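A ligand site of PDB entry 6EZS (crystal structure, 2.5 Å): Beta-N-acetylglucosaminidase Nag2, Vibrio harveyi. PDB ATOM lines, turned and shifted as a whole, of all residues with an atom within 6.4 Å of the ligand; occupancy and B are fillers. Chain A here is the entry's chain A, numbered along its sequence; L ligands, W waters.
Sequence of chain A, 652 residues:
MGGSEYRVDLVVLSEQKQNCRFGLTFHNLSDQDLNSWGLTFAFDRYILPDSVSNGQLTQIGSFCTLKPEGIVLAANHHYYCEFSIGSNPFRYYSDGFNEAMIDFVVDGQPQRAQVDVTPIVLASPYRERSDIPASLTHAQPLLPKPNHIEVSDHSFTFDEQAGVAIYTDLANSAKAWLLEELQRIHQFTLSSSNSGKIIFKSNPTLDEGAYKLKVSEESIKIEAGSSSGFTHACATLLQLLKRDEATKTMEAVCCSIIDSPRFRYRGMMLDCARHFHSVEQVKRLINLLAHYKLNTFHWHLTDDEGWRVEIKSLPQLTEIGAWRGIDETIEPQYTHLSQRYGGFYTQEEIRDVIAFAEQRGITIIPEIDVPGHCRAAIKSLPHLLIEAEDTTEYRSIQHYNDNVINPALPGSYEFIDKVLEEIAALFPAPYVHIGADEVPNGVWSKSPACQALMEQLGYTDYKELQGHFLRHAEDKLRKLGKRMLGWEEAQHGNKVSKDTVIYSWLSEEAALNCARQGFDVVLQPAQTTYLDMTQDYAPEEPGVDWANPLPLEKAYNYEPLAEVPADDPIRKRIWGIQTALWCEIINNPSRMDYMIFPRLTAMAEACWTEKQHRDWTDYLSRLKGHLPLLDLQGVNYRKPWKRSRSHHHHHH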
ATOM      1  N   ASP A 271     -14.075   6.268   9.165  1.00  0.00           N
ATOM      2  CA  ASP A 271     -15.145   5.970  10.119  1.00  0.00           C
ATOM      3  C   ASP A 271     -15.649   7.233  10.820  1.00  0.00           C
ATOM      4  O   ASP A 271     -14.976   7.736  11.714  1.00  0.00           O
ATOM      5  CB  ASP A 271     -14.622   4.962  11.162  1.00  0.00           C
ATOM      6  CG  ASP A 271     -15.660   4.602  12.220  1.00  0.00           C
ATOM      7  OD1 ASP A 271     -16.828   5.029  12.110  1.00  0.00           O
ATOM      8  OD2 ASP A 271     -15.281   3.877  13.168  1.00  0.00           O
ATOM      9  N   ARG A 274     -18.366   6.021  14.627  1.00  0.00           N
ATOM     10  CA  ARG A 274     -17.829   5.853  15.980  1.00  0.00           C
ATOM     11  C   ARG A 274     -17.599   7.190  16.671  1.00  0.00           C
ATOM     12  O   ARG A 274     -17.909   7.345  17.832  1.00  0.00           O
ATOM     13  CB  ARG A 274     -16.535   5.046  15.973  1.00  0.00           C
ATOM     14  CG  ARG A 274     -16.728   3.544  15.912  1.00  0.00           C
ATOM     15  CD  ARG A 274     -17.843   3.090  14.964  1.00  0.00           C
ATOM     16  NE  ARG A 274     -18.021   1.640  14.995  1.00  0.00           N
ATOM     17  CZ  ARG A 274     -17.235   0.761  14.384  1.00  0.00           C
ATOM     18  NH1 ARG A 274     -16.191   1.162  13.639  1.00  0.00           N
ATOM     19  NH2 ARG A 274     -17.497  -0.540  14.519  1.00  0.00           N
ATOM     20  N   HIS A 300     -17.782   6.079   5.747  1.00  0.00           N
ATOM     21  CA  HIS A 300     -18.447   5.166   6.645  1.00  0.00           C
ATOM     22  C   HIS A 300     -19.379   5.979   7.563  1.00  0.00           C
ATOM     23  O   HIS A 300     -18.960   6.448   8.627  1.00  0.00           O
ATOM     24  CB  HIS A 300     -17.424   4.361   7.432  1.00  0.00           C
ATOM     25  CG  HIS A 300     -18.014   3.229   8.207  1.00  0.00           C
ATOM     26  ND1 HIS A 300     -18.427   2.067   7.607  1.00  0.00           N
ATOM     27  CD2 HIS A 300     -18.300   3.091   9.523  1.00  0.00           C
ATOM     28  CE1 HIS A 300     -18.940   1.251   8.511  1.00  0.00           C
ATOM     29  NE2 HIS A 300     -18.880   1.853   9.684  1.00  0.00           N
ATOM     30  N   ASP A 303     -23.196   3.173  11.725  1.00  0.00           N
ATOM     31  CA  ASP A 303     -22.712   2.019  12.477  1.00  0.00           C
ATOM     32  C   ASP A 303     -23.585   1.892  13.722  1.00  0.00           C
ATOM     33  O   ASP A 303     -24.610   2.578  13.820  1.00  0.00           O
ATOM     34  CB  ASP A 303     -21.211   2.165  12.823  1.00  0.00           C
ATOM     35  CG  ASP A 303     -20.450   0.832  12.740  1.00  0.00           C
ATOM     36  OD1 ASP A 303     -20.924  -0.163  13.340  1.00  0.00           O
ATOM     37  OD2 ASP A 303     -19.404   0.760  12.066  1.00  0.00           O
ATOM     38  N   GLU A 367     -21.560   4.543   2.600  1.00  0.00           N
ATOM     39  CA  GLU A 367     -21.798   3.214   3.168  1.00  0.00           C
ATOM     40  C   GLU A 367     -22.909   3.278   4.161  1.00  0.00           C
ATOM     41  O   GLU A 367     -22.863   4.056   5.095  1.00  0.00           O
ATOM     42  CB  GLU A 367     -20.562   2.625   3.852  1.00  0.00           C
ATOM     43  CG  GLU A 367     -20.781   1.200   4.377  1.00  0.00           C
ATOM     44  CD  GLU A 367     -19.596   0.632   5.137  1.00  0.00           C
ATOM     45  OE1 GLU A 367     -18.447   1.087   4.934  1.00  0.00           O
ATOM     46  OE2 GLU A 367     -19.783  -0.280   5.967  1.00  0.00           O
ATOM     47  N   HIS A 373     -24.639  -4.258  12.236  1.00  0.00           N
ATOM     48  CA  HIS A 373     -24.144  -2.926  12.590  1.00  0.00           C
ATOM     49  C   HIS A 373     -25.224  -1.823  12.484  1.00  0.00           C
ATOM     50  O   HIS A 373     -24.948  -0.707  12.067  1.00  0.00           O
ATOM     51  CB  HIS A 373     -22.896  -2.560  11.770  1.00  0.00           C
ATOM     52  CG  HIS A 373     -21.675  -3.330  12.151  1.00  0.00           C
ATOM     53  ND1 HIS A 373     -20.723  -2.833  13.006  1.00  0.00           N
ATOM     54  CD2 HIS A 373     -21.252  -4.558  11.767  1.00  0.00           C
ATOM     55  CE1 HIS A 373     -19.749  -3.726  13.139  1.00  0.00           C
ATOM     56  NE2 HIS A 373     -20.048  -4.780  12.399  1.00  0.00           N
ATOM     57  N   GLN A 398     -18.891  -6.687  18.664  1.00  0.00           N
ATOM     58  CA  GLN A 398     -18.728  -5.428  19.412  1.00  0.00           C
ATOM     59  C   GLN A 398     -19.589  -5.373  20.691  1.00  0.00           C
ATOM     60  O   GLN A 398     -19.863  -4.297  21.182  1.00  0.00           O
ATOM     61  CB  GLN A 398     -19.039  -4.226  18.504  1.00  0.00           C
ATOM     62  CG  GLN A 398     -17.993  -3.939  17.419  1.00  0.00           C
ATOM     63  CD  GLN A 398     -18.020  -4.892  16.211  1.00  0.00           C
ATOM     64  OE1 GLN A 398     -19.013  -5.584  15.942  1.00  0.00           O
ATOM     65  NE2 GLN A 398     -16.898  -4.919  15.465  1.00  0.00           N
ATOM     66  N   ASP A 437     -21.829  -7.113   6.594  1.00  0.00           N
ATOM     67  CA  ASP A 437     -21.054  -7.756   7.640  1.00  0.00           C
ATOM     68  C   ASP A 437     -21.738  -9.049   8.048  1.00  0.00           C
ATOM     69  O   ASP A 437     -22.982  -9.154   8.008  1.00  0.00           O
ATOM     70  CB  ASP A 437     -20.942  -6.875   8.897  1.00  0.00           C
ATOM     71  CG  ASP A 437     -20.225  -5.562   8.638  1.00  0.00           C
ATOM     72  OD1 ASP A 437     -20.881  -4.636   8.071  1.00  0.00           O
ATOM     73  OD2 ASP A 437     -19.034  -5.435   9.015  1.00  0.00           O
ATOM     74  N   TRP A 487     -18.556  -5.762   2.116  1.00  0.00           N
ATOM     75  CA  TRP A 487     -17.400  -6.360   2.768  1.00  0.00           C
ATOM     76  C   TRP A 487     -17.376  -7.845   2.455  1.00  0.00           C
ATOM     77  O   TRP A 487     -18.416  -8.438   2.164  1.00  0.00           O
ATOM     78  CB  TRP A 487     -17.441  -6.185   4.273  1.00  0.00           C
ATOM     79  CG  TRP A 487     -17.410  -4.762   4.768  1.00  0.00           C
ATOM     80  CD1 TRP A 487     -18.381  -4.152   5.523  1.00  0.00           C
ATOM     81  CD2 TRP A 487     -16.375  -3.791   4.573  1.00  0.00           C
ATOM     82  NE1 TRP A 487     -18.013  -2.853   5.798  1.00  0.00           N
ATOM     83  CE2 TRP A 487     -16.789  -2.605   5.234  1.00  0.00           C
ATOM     84  CE3 TRP A 487     -15.126  -3.805   3.915  1.00  0.00           C
ATOM     85  CZ2 TRP A 487     -16.021  -1.451   5.242  1.00  0.00           C
ATOM     86  CZ3 TRP A 487     -14.355  -2.642   3.900  1.00  0.00           C
ATOM     87  CH2 TRP A 487     -14.814  -1.479   4.568  1.00  0.00           C
ATOM     88  N   TRP A 505     -10.629  -7.834   3.397  1.00  0.00           N
ATOM     89  CA  TRP A 505      -9.648  -7.517   4.451  1.00  0.00           C
ATOM     90  C   TRP A 505      -8.904  -8.709   5.051  1.00  0.00           C
ATOM     91  O   TRP A 505      -7.955  -8.510   5.789  1.00  0.00           O
ATOM     92  CB  TRP A 505     -10.284  -6.713   5.582  1.00  0.00           C
ATOM     93  CG  TRP A 505     -11.051  -7.525   6.558  1.00  0.00           C
ATOM     94  CD1 TRP A 505     -10.552  -8.381   7.507  1.00  0.00           C
ATOM     95  CD2 TRP A 505     -12.466  -7.524   6.722  1.00  0.00           C
ATOM     96  NE1 TRP A 505     -11.579  -8.938   8.230  1.00  0.00           N
ATOM     97  CE2 TRP A 505     -12.766  -8.419   7.773  1.00  0.00           C
ATOM     98  CE3 TRP A 505     -13.513  -6.873   6.070  1.00  0.00           C
ATOM     99  CZ2 TRP A 505     -14.045  -8.654   8.176  1.00  0.00           C
ATOM    100  CZ3 TRP A 505     -14.766  -7.111   6.485  1.00  0.00           C
ATOM    101  CH2 TRP A 505     -15.037  -8.001   7.524  1.00  0.00           C
ATOM    102  N   ALA A 526      -6.531  -6.089   6.721  1.00  0.00           N
ATOM    103  CA  ALA A 526      -6.436  -5.596   8.104  1.00  0.00           C
ATOM    104  C   ALA A 526      -5.003  -5.484   8.618  1.00  0.00           C
ATOM    105  O   ALA A 526      -4.660  -4.501   9.284  1.00  0.00           O
ATOM    106  CB  ALA A 526      -7.263  -6.482   9.048  1.00  0.00           C
ATOM    107  N   TYR A 530      -4.898  -0.942   8.025  1.00  0.00           N
ATOM    108  CA  TYR A 530      -5.703  -0.365   9.111  1.00  0.00           C
ATOM    109  C   TYR A 530      -4.884   0.637   9.906  1.00  0.00           C
ATOM    110  O   TYR A 530      -4.070   0.264  10.749  1.00  0.00           O
ATOM    111  CB  TYR A 530      -6.234  -1.461  10.036  1.00  0.00           C
ATOM    112  CG  TYR A 530      -7.488  -2.199   9.559  1.00  0.00           C
ATOM    113  CD1 TYR A 530      -7.839  -2.254   8.219  1.00  0.00           C
ATOM    114  CD2 TYR A 530      -8.291  -2.867  10.467  1.00  0.00           C
ATOM    115  CE1 TYR A 530      -8.954  -2.941   7.816  1.00  0.00           C
ATOM    116  CE2 TYR A 530      -9.381  -3.567  10.075  1.00  0.00           C
ATOM    117  CZ  TYR A 530      -9.717  -3.604   8.741  1.00  0.00           C
ATOM    118  OH  TYR A 530     -10.838  -4.299   8.351  1.00  0.00           O
ATOM    119  N   ASP A 532      -5.890   2.549  12.230  1.00  0.00           N
ATOM    120  CA  ASP A 532      -6.210   2.564  13.662  1.00  0.00           C
ATOM    121  C   ASP A 532      -5.221   1.766  14.496  1.00  0.00           C
ATOM    122  O   ASP A 532      -5.174   1.917  15.726  1.00  0.00           O
ATOM    123  CB  ASP A 532      -7.667   2.142  13.982  1.00  0.00           C
ATOM    124  CG  ASP A 532      -8.048   0.754  13.449  1.00  0.00           C
ATOM    125  OD1 ASP A 532      -7.697   0.431  12.299  1.00  0.00           O
ATOM    126  OD2 ASP A 532      -8.741   0.011  14.180  1.00  0.00           O
ATOM    127  N   MET A 533      -4.414   0.942  13.835  1.00  0.00           N
ATOM    128  CA  MET A 533      -3.400   0.176  14.507  1.00  0.00           C
ATOM    129  C   MET A 533      -2.233   1.049  14.981  1.00  0.00           C
ATOM    130  O   MET A 533      -1.822   1.980  14.286  1.00  0.00           O
ATOM    131  CB  MET A 533      -2.863  -0.918  13.604  1.00  0.00           C
ATOM    132  CG  MET A 533      -3.882  -1.935  13.173  1.00  0.00           C
ATOM    133  SD  MET A 533      -4.514  -2.865  14.577  1.00  0.00           S
ATOM    134  CE  MET A 533      -6.250  -2.661  14.175  1.00  0.00           C
ATOM    135  N   VAL A 544      -4.925   0.713  18.479  1.00  0.00           N
ATOM    136  CA  VAL A 544      -5.270  -0.656  18.863  1.00  0.00           C
ATOM    137  C   VAL A 544      -4.274  -1.574  18.142  1.00  0.00           C
ATOM    138  O   VAL A 544      -3.521  -1.120  17.281  1.00  0.00           O
ATOM    139  CB  VAL A 544      -6.755  -0.976  18.548  1.00  0.00           C
ATOM    140  CG1 VAL A 544      -7.664   0.124  19.086  1.00  0.00           C
ATOM    141  CG2 VAL A 544      -7.006  -1.154  17.055  1.00  0.00           C
ATOM    142  N   TRP A 546      -5.061  -5.360  17.600  1.00  0.00           N
ATOM    143  CA  TRP A 546      -5.618  -6.724  17.477  1.00  0.00           C
ATOM    144  C   TRP A 546      -5.117  -7.410  16.210  1.00  0.00           C
ATOM    145  O   TRP A 546      -4.830  -8.590  16.241  1.00  0.00           O
ATOM    146  CB  TRP A 546      -7.151  -6.727  17.570  1.00  0.00           C
ATOM    147  CG  TRP A 546      -7.838  -6.122  16.410  1.00  0.00           C
ATOM    148  CD1 TRP A 546      -8.209  -4.811  16.255  1.00  0.00           C
ATOM    149  CD2 TRP A 546      -8.220  -6.795  15.206  1.00  0.00           C
ATOM    150  NE1 TRP A 546      -8.812  -4.628  15.027  1.00  0.00           N
ATOM    151  CE2 TRP A 546      -8.822  -5.828  14.357  1.00  0.00           C
ATOM    152  CE3 TRP A 546      -8.092  -8.121  14.735  1.00  0.00           C
ATOM    153  CZ2 TRP A 546      -9.315  -6.151  13.080  1.00  0.00           C
ATOM    154  CZ3 TRP A 546      -8.571  -8.436  13.463  1.00  0.00           C
ATOM    155  CH2 TRP A 546      -9.183  -7.455  12.662  1.00  0.00           C
ATOM    156  N   TRP A 582     -10.484   3.393  11.449  1.00  0.00           N
ATOM    157  CA  TRP A 582     -11.588   3.088  12.352  1.00  0.00           C
ATOM    158  C   TRP A 582     -11.402   3.966  13.578  1.00  0.00           C
ATOM    159  O   TRP A 582     -10.285   4.178  14.032  1.00  0.00           O
ATOM    160  CB  TRP A 582     -11.580   1.599  12.685  1.00  0.00           C
ATOM    161  CG  TRP A 582     -11.680   0.778  11.457  1.00  0.00           C
ATOM    162  CD1 TRP A 582     -10.661   0.123  10.810  1.00  0.00           C
ATOM    163  CD2 TRP A 582     -12.865   0.535  10.673  1.00  0.00           C
ATOM    164  NE1 TRP A 582     -11.142  -0.530   9.702  1.00  0.00           N
ATOM    165  CE2 TRP A 582     -12.485  -0.287   9.594  1.00  0.00           C
ATOM    166  CE3 TRP A 582     -14.194   0.936  10.792  1.00  0.00           C
ATOM    167  CZ2 TRP A 582     -13.402  -0.722   8.639  1.00  0.00           C
ATOM    168  CZ3 TRP A 582     -15.105   0.490   9.856  1.00  0.00           C
ATOM    169  CH2 TRP A 582     -14.707  -0.324   8.791  1.00  0.00           C
ATOM    170  N   CYS A 583     -12.500   4.516  14.082  1.00  0.00           N
ATOM    171  CA  CYS A 583     -12.410   5.671  14.987  1.00  0.00           C
ATOM    172  C   CYS A 583     -12.920   5.441  16.383  1.00  0.00           C
ATOM    173  O   CYS A 583     -13.293   6.408  17.053  1.00  0.00           O
ATOM    174  CB  CYS A 583     -13.083   6.881  14.338  1.00  0.00           C
ATOM    175  SG  CYS A 583     -12.037   7.555  13.037  1.00  0.00           S
ATOM    176  N   GLU A 584     -12.834   4.198  16.852  1.00  0.00           N
ATOM    177  CA  GLU A 584     -13.206   3.834  18.241  1.00  0.00           C
ATOM    178  C   GLU A 584     -12.515   4.695  19.290  1.00  0.00           C
ATOM    179  O   GLU A 584     -13.112   5.031  20.294  1.00  0.00           O
ATOM    180  CB  GLU A 584     -12.867   2.373  18.567  1.00  0.00           C
ATOM    181  CG  GLU A 584     -13.815   1.330  18.030  1.00  0.00           C
ATOM    182  CD  GLU A 584     -13.524   0.935  16.610  1.00  0.00           C
ATOM    183  OE1 GLU A 584     -12.815   1.676  15.894  1.00  0.00           O
ATOM    184  OE2 GLU A 584     -14.018  -0.136  16.199  1.00  0.00           O
HETATM  185  C1  LIG L   1     -12.601  -3.941  11.386  1.00  0.00           C
HETATM  186  C2  LIG L   1     -14.133  -3.810  11.527  1.00  0.00           C
HETATM  187  C3  LIG L   1     -14.589  -2.524  12.229  1.00  0.00           C
HETATM  188  C4  LIG L   1     -13.755  -2.197  13.452  1.00  0.00           C
HETATM  189  C5  LIG L   1     -12.285  -2.476  13.171  1.00  0.00           C
HETATM  190  C6  LIG L   1     -11.403  -2.277  14.404  1.00  0.00           C
HETATM  191  C7  LIG L   1     -15.671  -4.604   9.715  1.00  0.00           C
HETATM  192  C8  LIG L   1     -16.072  -4.288   8.309  1.00  0.00           C
HETATM  193  N1  LIG L   1     -14.712  -3.789  10.164  1.00  0.00           N
HETATM  194  O1  LIG L   1     -12.209  -5.219  10.895  1.00  0.00           O
HETATM  195  O2  LIG L   1     -15.945  -2.645  12.636  1.00  0.00           O
HETATM  196  O3  LIG L   1     -13.995  -0.830  13.743  1.00  0.00           O
HETATM  197  O4  LIG L   1     -12.189  -3.815  12.735  1.00  0.00           O
HETATM  198  O5  LIG L   1     -10.049  -2.177  13.976  1.00  0.00           O
HETATM  199  O6  LIG L   1     -16.179  -5.500  10.375  1.00  0.00           O
HETATM  200  O   HOH W   1     -12.715  -6.135  14.293  1.00  0.00           O
HETATM  201  O   HOH W   2     -17.128  -5.705  12.993  1.00  0.00           O
HETATM  202  O   HOH W   3     -18.261  -1.549  11.104  1.00  0.00           O
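An oxygen (O6) of the ligand lies close to the side-chain carboxylate (OD2) of Asp 437. His 373 touches the ligand. Gln 398 touches the ligand (NE2 to O2, 3.8 Å). NE1 of Trp 487 touches C8 of the ligand (3.5 Å). Trp 505 touches the ligand. Met 533 touches the ligand (CE to O5, 3.8 Å). Trp 582 touches the ligand. Within 4 Å of the ligand: Arg 274, His 373, Gln 398, Asp 437, Trp 487, Trp 505, Tyr 530, Asp 532, Met 533, Trp 546, Trp 582 and Glu 584. The nearest printed residue that does not touch the ligand is Val 544 (4.4 Å).
An oxygen (O3) of the ligand sits at hydrogen-bond distance from the guanidinium group (NH1) of Arg 274, 3.0 Å away. The side-chain carboxylate (OD2) of Asp 532 lies within hydrogen-bond range of an oxygen (O5) of the ligand, at 2.6 Å. OH of Tyr 530 is in hydrogen-bond range of O1 of the ligand. O5 of the ligand is in hydrogen-bond range of NE1 of Trp 546 (2.9 Å). The side-chain carboxylate of Glu 584 lies within hydrogen-bond range of an oxygen (O3) of the ligand.
Water W2 lies within hydrogen-bond range of the side-chain amide nitrogen of Gln 398 (2.6 Å), an oxygen (O6) of the ligand (2.8 Å) and a ring nitrogen (NE2) of His 373 (3.1 Å). Water W3 lies within hydrogen-bond range of OD2 of Asp 303 (2.8 Å), O2 of the ligand (3.0 Å) and ND1 of His 373 (3.4 Å).
The side-chain carboxylate (OE2) of Glu 584 lies within salt-bridge range of the guanidinium group (NH1) of Arg 274. The backbone carbonyl oxygen (O) of Trp 505 lies within hydrogen-bond range of the backbone NH (N) of Ala 526 (3.0 Å). The guanidinium group (NE) of Arg 274 is in salt-bridge range of the side-chain carboxylate (OD2) of Asp 303 (3.4 Å). A ring nitrogen (ND1) of His 373 is in hydrogen-bond range of the side-chain carboxylate (OD1) of Asp 303, at 2.7 Å. The backbone carbonyl oxygen (O) of Asp 532 sits at hydrogen-bond distance from the backbone NH (N) of Val 544. NE1 of Trp 487 is in hydrogen-bond range of OE2 of Glu 367, 3.1 Å away. The guanidinium group of Arg 274 lies within salt-bridge range of the side-chain carboxylate of Asp 271, 2.9 Å away.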
